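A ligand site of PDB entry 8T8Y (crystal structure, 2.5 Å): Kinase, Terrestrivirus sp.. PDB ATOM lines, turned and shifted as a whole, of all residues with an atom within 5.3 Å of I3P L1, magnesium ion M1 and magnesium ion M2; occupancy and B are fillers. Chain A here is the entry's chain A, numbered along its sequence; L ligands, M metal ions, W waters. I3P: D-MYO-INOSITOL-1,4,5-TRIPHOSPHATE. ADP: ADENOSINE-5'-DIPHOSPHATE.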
ATOM      1  N   GLY A  41     -14.227  30.360 -19.160  1.00  0.00           N
ATOM      2  CA  GLY A  41     -15.252  31.417 -19.246  1.00  0.00           C
ATOM      3  C   GLY A  41     -14.943  32.416 -20.344  1.00  0.00           C
ATOM      4  O   GLY A  41     -14.181  32.061 -21.260  1.00  0.00           O
ATOM      5  N   ARG A  42     -15.525  33.620 -20.262  1.00  0.00           N
ATOM      6  CA  ARG A  42     -15.478  34.626 -21.351  1.00  0.00           C
ATOM      7  C   ARG A  42     -15.597  36.067 -20.821  1.00  0.00           C
ATOM      8  O   ARG A  42     -15.354  36.989 -21.618  1.00  0.00           O
ATOM      9  CB  ARG A  42     -16.602  34.337 -22.341  1.00  0.00           C
ATOM     10  CG  ARG A  42     -18.008  34.491 -21.756  1.00  0.00           C
ATOM     11  CD  ARG A  42     -18.979  33.460 -22.303  1.00  0.00           C
ATOM     12  NE  ARG A  42     -18.508  32.116 -21.989  1.00  0.00           N
ATOM     13  CZ  ARG A  42     -18.021  31.224 -22.866  1.00  0.00           C
ATOM     14  NH1 ARG A  42     -17.951  31.517 -24.155  1.00  0.00           N
ATOM     15  NH2 ARG A  42     -17.615  30.042 -22.442  1.00  0.00           N
ATOM     16  N   LYS A  60     -25.485  41.607 -19.216  1.00  0.00           N
ATOM     17  CA  LYS A  60     -26.944  41.300 -19.260  1.00  0.00           C
ATOM     18  C   LYS A  60     -27.672  41.989 -18.101  1.00  0.00           C
ATOM     19  O   LYS A  60     -28.650  42.699 -18.378  1.00  0.00           O
ATOM     20  CB  LYS A  60     -27.209  39.792 -19.238  1.00  0.00           C
ATOM     21  CG  LYS A  60     -26.433  38.975 -20.267  1.00  0.00           C
ATOM     22  CD  LYS A  60     -27.028  37.591 -20.498  1.00  0.00           C
ATOM     23  CE  LYS A  60     -26.455  36.882 -21.699  1.00  0.00           C
ATOM     24  NZ  LYS A  60     -24.989  36.678 -21.573  1.00  0.00           N
ATOM     25  N   ASP A 110     -11.229  25.152 -13.498  1.00  0.00           N
ATOM     26  CA  ASP A 110     -12.663  25.530 -13.461  1.00  0.00           C
ATOM     27  C   ASP A 110     -13.465  24.269 -13.822  1.00  0.00           C
ATOM     28  O   ASP A 110     -13.265  23.767 -14.943  1.00  0.00           O
ATOM     29  CB  ASP A 110     -12.919  26.682 -14.425  1.00  0.00           C
ATOM     30  CG  ASP A 110     -14.345  27.240 -14.417  1.00  0.00           C
ATOM     31  OD1 ASP A 110     -15.286  26.414 -14.270  1.00  0.00           O
ATOM     32  OD2 ASP A 110     -14.495  28.499 -14.604  1.00  0.00           O
ATOM     33  N   LYS A 112     -17.481  23.063 -14.011  1.00  0.00           N
ATOM     34  CA  LYS A 112     -18.903  23.496 -14.017  1.00  0.00           C
ATOM     35  C   LYS A 112     -19.729  22.403 -13.340  1.00  0.00           C
ATOM     36  O   LYS A 112     -19.745  21.278 -13.859  1.00  0.00           O
ATOM     37  CB  LYS A 112     -19.297  23.727 -15.475  1.00  0.00           C
ATOM     38  CG  LYS A 112     -20.719  24.160 -15.755  1.00  0.00           C
ATOM     39  CD  LYS A 112     -20.925  25.630 -15.551  1.00  0.00           C
ATOM     40  CE  LYS A 112     -20.520  26.489 -16.726  1.00  0.00           C
ATOM     41  NZ  LYS A 112     -21.196  27.811 -16.660  1.00  0.00           N
ATOM     42  N   ALA A 115     -26.221  23.408 -13.545  1.00  0.00           N
ATOM     43  CA  ALA A 115     -26.835  23.103 -14.866  1.00  0.00           C
ATOM     44  C   ALA A 115     -26.292  24.075 -15.906  1.00  0.00           C
ATOM     45  O   ALA A 115     -26.161  25.288 -15.600  1.00  0.00           O
ATOM     46  CB  ALA A 115     -28.341  23.164 -14.798  1.00  0.00           C
ATOM     47  N   ARG A 116     -25.981  23.546 -17.091  1.00  0.00           N
ATOM     48  CA  ARG A 116     -25.649  24.328 -18.311  1.00  0.00           C
ATOM     49  C   ARG A 116     -26.930  24.923 -18.897  1.00  0.00           C
ATOM     50  O   ARG A 116     -27.993  24.323 -18.703  1.00  0.00           O
ATOM     51  CB  ARG A 116     -24.965  23.410 -19.316  1.00  0.00           C
ATOM     52  CG  ARG A 116     -23.755  22.687 -18.738  1.00  0.00           C
ATOM     53  CD  ARG A 116     -22.822  22.211 -19.826  1.00  0.00           C
ATOM     54  NE  ARG A 116     -22.327  23.311 -20.621  1.00  0.00           N
ATOM     55  CZ  ARG A 116     -21.550  23.192 -21.697  1.00  0.00           C
ATOM     56  NH1 ARG A 116     -21.163  21.998 -22.110  1.00  0.00           N
ATOM     57  NH2 ARG A 116     -21.172  24.278 -22.341  1.00  0.00           N
ATOM     58  N   LYS A 117     -26.834  26.070 -19.573  1.00  0.00           N
ATOM     59  CA  LYS A 117     -27.974  26.775 -20.210  1.00  0.00           C
ATOM     60  C   LYS A 117     -28.644  25.888 -21.270  1.00  0.00           C
ATOM     61  O   LYS A 117     -29.880  25.759 -21.209  1.00  0.00           O
ATOM     62  CB  LYS A 117     -27.508  28.079 -20.869  1.00  0.00           C
ATOM     63  CG  LYS A 117     -28.033  29.358 -20.233  1.00  0.00           C
ATOM     64  CD  LYS A 117     -29.215  29.957 -20.945  1.00  0.00           C
ATOM     65  CE  LYS A 117     -28.854  31.119 -21.840  1.00  0.00           C
ATOM     66  NZ  LYS A 117     -28.970  32.415 -21.130  1.00  0.00           N
ATOM     67  N   ARG A 118     -27.866  25.325 -22.202  1.00  0.00           N
ATOM     68  CA  ARG A 118     -28.392  24.774 -23.474  1.00  0.00           C
ATOM     69  C   ARG A 118     -27.873  23.359 -23.767  1.00  0.00           C
ATOM     70  O   ARG A 118     -28.631  22.603 -24.367  1.00  0.00           O
ATOM     71  CB  ARG A 118     -28.070  25.734 -24.633  1.00  0.00           C
ATOM     72  CG  ARG A 118     -29.090  26.862 -24.764  1.00  0.00           C
ATOM     73  CD  ARG A 118     -28.868  27.773 -25.954  1.00  0.00           C
ATOM     74  NE  ARG A 118     -28.126  28.955 -25.549  1.00  0.00           N
ATOM     75  CZ  ARG A 118     -28.663  30.134 -25.242  1.00  0.00           C
ATOM     76  NH1 ARG A 118     -29.966  30.349 -25.332  1.00  0.00           N
ATOM     77  NH2 ARG A 118     -27.861  31.118 -24.853  1.00  0.00           N
ATOM     78  N   ARG A 129     -14.102  23.048 -17.465  1.00  0.00           N
ATOM     79  CA  ARG A 129     -14.228  24.212 -18.377  1.00  0.00           C
ATOM     80  C   ARG A 129     -12.843  24.682 -18.830  1.00  0.00           C
ATOM     81  O   ARG A 129     -12.774  25.369 -19.835  1.00  0.00           O
ATOM     82  CB  ARG A 129     -14.972  25.377 -17.726  1.00  0.00           C
ATOM     83  CG  ARG A 129     -16.360  25.017 -17.229  1.00  0.00           C
ATOM     84  CD  ARG A 129     -17.126  24.125 -18.176  1.00  0.00           C
ATOM     85  NE  ARG A 129     -17.335  24.719 -19.487  1.00  0.00           N
ATOM     86  CZ  ARG A 129     -17.247  24.069 -20.649  1.00  0.00           C
ATOM     87  NH1 ARG A 129     -17.481  24.705 -21.772  1.00  0.00           N
ATOM     88  NH2 ARG A 129     -16.901  22.784 -20.692  1.00  0.00           N
ATOM     89  N   GLY A 195     -25.045  27.037 -13.657  1.00  0.00           N
ATOM     90  CA  GLY A 195     -23.816  27.551 -14.277  1.00  0.00           C
ATOM     91  C   GLY A 195     -22.653  27.722 -13.309  1.00  0.00           C
ATOM     92  O   GLY A 195     -21.573  28.054 -13.818  1.00  0.00           O
ATOM     93  N   SER A 197     -19.360  27.245 -11.016  1.00  0.00           N
ATOM     94  CA  SER A 197     -18.127  26.457 -11.179  1.00  0.00           C
ATOM     95  C   SER A 197     -17.417  26.324  -9.826  1.00  0.00           C
ATOM     96  O   SER A 197     -17.545  27.230  -9.000  1.00  0.00           O
ATOM     97  CB  SER A 197     -17.232  27.067 -12.224  1.00  0.00           C
ATOM     98  OG  SER A 197     -17.795  26.896 -13.527  1.00  0.00           O
ATOM     99  N   ASP A 215     -19.225  32.301 -10.184  1.00  0.00           N
ATOM    100  CA  ASP A 215     -20.162  32.549 -11.309  1.00  0.00           C
ATOM    101  C   ASP A 215     -21.606  32.319 -10.843  1.00  0.00           C
ATOM    102  O   ASP A 215     -22.166  31.239 -11.089  1.00  0.00           O
ATOM    103  CB  ASP A 215     -19.819  31.713 -12.553  1.00  0.00           C
ATOM    104  CG  ASP A 215     -20.415  32.234 -13.852  1.00  0.00           C
ATOM    105  OD1 ASP A 215     -21.273  33.156 -13.778  1.00  0.00           O
ATOM    106  OD2 ASP A 215     -20.021  31.728 -14.951  1.00  0.00           O
ATOM    107  N   ARG A 218     -26.206  33.222 -13.316  1.00  0.00           N
ATOM    108  CA  ARG A 218     -27.433  32.530 -13.795  1.00  0.00           C
ATOM    109  C   ARG A 218     -28.113  31.781 -12.633  1.00  0.00           C
ATOM    110  O   ARG A 218     -29.013  30.966 -12.903  1.00  0.00           O
ATOM    111  CB  ARG A 218     -27.088  31.570 -14.940  1.00  0.00           C
ATOM    112  CG  ARG A 218     -26.478  32.249 -16.155  1.00  0.00           C
ATOM    113  CD  ARG A 218     -25.981  31.281 -17.228  1.00  0.00           C
ATOM    114  NE  ARG A 218     -26.833  30.099 -17.235  1.00  0.00           N
ATOM    115  CZ  ARG A 218     -26.435  28.830 -17.096  1.00  0.00           C
ATOM    116  NH1 ARG A 218     -25.162  28.506 -16.992  1.00  0.00           N
ATOM    117  NH2 ARG A 218     -27.356  27.883 -17.098  1.00  0.00           N
HETATM  118  C1  I3P L   1     -24.088  31.394 -21.392  1.00  0.00           C
HETATM  119  C2  I3P L   1     -22.943  32.389 -21.136  1.00  0.00           C
HETATM  120  C3  I3P L   1     -22.215  31.996 -19.876  1.00  0.00           C
HETATM  121  C4  I3P L   1     -21.631  30.588 -20.006  1.00  0.00           C
HETATM  122  C5  I3P L   1     -22.786  29.595 -20.207  1.00  0.00           C
HETATM  123  C6  I3P L   1     -23.539  29.979 -21.513  1.00  0.00           C
HETATM  124  O1  I3P L   1     -24.840  31.698 -22.587  1.00  0.00           O
HETATM  125  O2  I3P L   1     -22.014  32.394 -22.247  1.00  0.00           O
HETATM  126  O3  I3P L   1     -21.171  32.958 -19.622  1.00  0.00           O
HETATM  127  O4  I3P L   1     -20.917  30.271 -18.796  1.00  0.00           O
HETATM  128  O5  I3P L   1     -22.259  28.229 -20.263  1.00  0.00           O
HETATM  129  O6  I3P L   1     -24.668  29.118 -21.737  1.00  0.00           O
HETATM  130  P1  I3P L   1     -25.630  33.113 -22.840  1.00  0.00           P
HETATM  131  O11 I3P L   1     -26.406  33.224 -21.512  1.00  0.00           O
HETATM  132  O12 I3P L   1     -24.426  34.129 -23.027  1.00  0.00           O
HETATM  133  O13 I3P L   1     -26.447  32.988 -24.078  1.00  0.00           O
HETATM  134  P4  I3P L   1     -19.317  30.202 -18.759  1.00  0.00           P
HETATM  135  O41 I3P L   1     -19.094  29.780 -17.252  1.00  0.00           O
HETATM  136  O42 I3P L   1     -18.857  31.668 -19.082  1.00  0.00           O
HETATM  137  O43 I3P L   1     -18.906  29.168 -19.744  1.00  0.00           O
HETATM  138  P5  I3P L   1     -22.986  26.945 -19.580  1.00  0.00           P
HETATM  139  O51 I3P L   1     -23.104  27.428 -18.099  1.00  0.00           O
HETATM  140  O52 I3P L   1     -21.840  25.952 -19.986  1.00  0.00           O
HETATM  141  O53 I3P L   1     -24.212  26.958 -20.373  1.00  0.00           O
HETATM  142  PB  ADP L   2     -17.425  33.880 -16.728  1.00  0.00           P
HETATM  143  O1B ADP L   2     -17.825  32.412 -16.884  1.00  0.00           O
HETATM  144  O2B ADP L   2     -16.255  34.263 -17.583  1.00  0.00           O
HETATM  145  O3B ADP L   2     -18.581  34.816 -16.883  1.00  0.00           O
HETATM  146  PA  ADP L   2     -16.472  33.086 -13.999  1.00  0.00           P
HETATM  147  O1A ADP L   2     -16.850  31.671 -14.311  1.00  0.00           O
HETATM  148  O2A ADP L   2     -16.987  33.694 -12.740  1.00  0.00           O
HETATM  149  O3A ADP L   2     -16.924  34.067 -15.192  1.00  0.00           O
HETATM  150  O5' ADP L   2     -14.874  33.235 -14.059  1.00  0.00           O
HETATM  151  C5' ADP L   2     -14.172  32.647 -15.177  1.00  0.00           C
HETATM  152  C4' ADP L   2     -12.734  32.400 -14.802  1.00  0.00           C
HETATM  153  O4' ADP L   2     -12.211  33.519 -14.046  1.00  0.00           O
HETATM  154  C3' ADP L   2     -12.470  31.166 -13.926  1.00  0.00           C
HETATM  155  O3' ADP L   2     -12.308  30.033 -14.779  1.00  0.00           O
HETATM  156  C2' ADP L   2     -11.194  31.556 -13.164  1.00  0.00           C
HETATM  157  O2' ADP L   2     -10.010  31.222 -13.854  1.00  0.00           O
HETATM  158  C1' ADP L   2     -11.317  33.078 -13.049  1.00  0.00           C
HETATM  159  N9  ADP L   2     -11.869  33.550 -11.776  1.00  0.00           N
HETATM  160  C8  ADP L   2     -13.157  33.951 -11.541  1.00  0.00           C
HETATM  161  N7  ADP L   2     -13.357  34.366 -10.316  1.00  0.00           N
HETATM  162  C5  ADP L   2     -12.107  34.260  -9.715  1.00  0.00           C
HETATM  163  C6  ADP L   2     -11.665  34.570  -8.419  1.00  0.00           C
HETATM  164  N6  ADP L   2     -12.436  35.080  -7.475  1.00  0.00           N
HETATM  165  N1  ADP L   2     -10.352  34.367  -8.155  1.00  0.00           N
HETATM  166  C2  ADP L   2      -9.562  33.874  -9.117  1.00  0.00           C
HETATM  167  N3  ADP L   2      -9.882  33.542 -10.369  1.00  0.00           N
HETATM  168  C4  ADP L   2     -11.184  33.764 -10.610  1.00  0.00           C
HETATM  169 MG    MG M   1     -18.285  30.649 -15.533  1.00  0.00          MG
HETATM  170 MG    MG M   2     -23.206  34.905 -24.726  1.00  0.00          MG
HETATM  171  O   HOH W   1     -21.260  27.208 -23.342  1.00  0.00           O
HETATM  172  O   HOH W   2     -25.512  28.707 -24.218  1.00  0.00           O
HETATM  173  O   HOH W   3     -21.135  33.224 -17.102  1.00  0.00           O
HETATM  174  O   HOH W   4     -22.081  32.710 -24.907  1.00  0.00           O
HETATM  175  O   HOH W   5     -25.420  34.226 -19.350  1.00  0.00           O
HETATM  176  O   HOH W   6     -24.874  34.298 -25.686  1.00  0.00           O
HETATM  177  O   HOH W   7     -21.719  35.551 -23.376  1.00  0.00           O
HETATM  178  O   HOH W   8     -21.464  35.618 -20.721  1.00  0.00           O
HETATM  179  O   HOH W   9     -16.622  28.243 -18.801  1.00  0.00           O
HETATM  180  O   HOH W  10     -18.994  29.026 -14.558  1.00  0.00           O
HETATM  181  O   HOH W  11     -24.442  36.749 -24.952  1.00  0.00           O
HETATM  182  O   HOH W  12     -16.702  29.294 -16.267  1.00  0.00           O
HETATM  183  O   HOH W  13     -23.593  34.033 -17.510  1.00  0.00           O
HETATM  184  O   HOH W  14     -25.028  25.289 -22.301  1.00  0.00           O
HETATM  185  O   HOH W  15     -22.985  30.547 -16.049  1.00  0.00           O
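The side-chain amino group of Lys 117 lies within salt-bridge range of an oxygen (O11) of I3P L1, 2.7 Å away.
The side-chain amino group (NZ) of Lys 112 is in salt-bridge range of an oxygen (O51) of I3P L1, at 2.4 Å.
The guanidinium group (NE) of Arg 42 is in salt-bridge range of an oxygen (O42) of I3P L1 (3.0 Å).
NZ of Lys 60 is in salt-bridge range of O11 of I3P L1 (3.7 Å).
The guanidinium group (NH1) of Arg 218 is in salt-bridge range of an oxygen (O51) of I3P L1 (2.6 Å).
An oxygen (O13) of I3P L1 is in salt-bridge range of the guanidinium group (NH2) of Arg 118.
The side-chain carboxylate (OD2) of Asp 110 sits at hydrogen-bond distance from an oxygen (O3') of ADP L2, at 2.7 Å.
The backbone NH of Lys 117 lies within hydrogen-bond range of an oxygen (O53) of I3P L1 (2.9 Å).
An oxygen (O2B) of ADP L2 lies within hydrogen-bond range of the backbone NH of Arg 42, at 2.9 Å.
An oxygen (O52) of I3P L1 is in salt-bridge range of the guanidinium group of Arg 116 (2.8 Å).
The guanidinium group (NH2) of Arg 218 lies within hydrogen-bond range of the backbone carbonyl oxygen (O) of Ala 115, 3.2 Å away.
O of Ala 115 is in hydrogen-bond range of N of Gly 195 (2.8 Å).
NZ of Lys 112 is in hydrogen-bond range of O of Gly 195 (2.9 Å).
Merely in contact with I3P L1: Gly 41 and Gly 195.
One residue has an atom within 4 Å of magnesium ion M1: Asp 215.
The nearest printed residue that does not touch magnesium ion M1 is Lys 112 (4.2 Å).
No residue comes within 4 Å of magnesium ion M2.
Magnesium ion M1 is bound by water W10 (2.0 Å), O41 of I3P L1 (2.1 Å), OD2 of Asp 215 (2.1 Å), O1A of ADP L2 (2.1 Å), water W12 (2.2 Å) and O1B of ADP L2 (2.3 Å).
Magnesium ion M1 has six donor atoms within binding distance.
Magnesium ion M2 is bound by water W6 (2.0 Å), water W7 (2.1 Å), O12 of I3P L1 (2.2 Å), water W11 (2.2 Å) and water W4 (2.5 Å).
Water W10 lies within hydrogen-bond range of the side-chain hydroxyl (OG) of Ser 197 (2.7 Å), the backbone carbonyl oxygen (O) of Gly 195 (2.9 Å) and the side-chain amino group (NZ) of Lys 112 (3.3 Å).
Water W3 lies within hydrogen-bond range of an oxygen (O3) of I3P L1, an oxygen (O3B) of ADP L2 and the side-chain carboxylate of Asp 215.
Water W5 bridges O11 of I3P L1 (2.6 Å) and NZ of Lys 60 (3.3 Å).
Water W9 bridges O43 of I3P L1 (2.6 Å) and N of Gly 41 (3.2 Å).
Water W1 bridges the guanidinium group of Arg 116 (3.1 Å) and an oxygen (O5) of I3P L1 (3.4 Å).
Water W15 lies within hydrogen-bond range of NH1 of Arg 218, NZ of Lys 112 and O4 of I3P L1.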
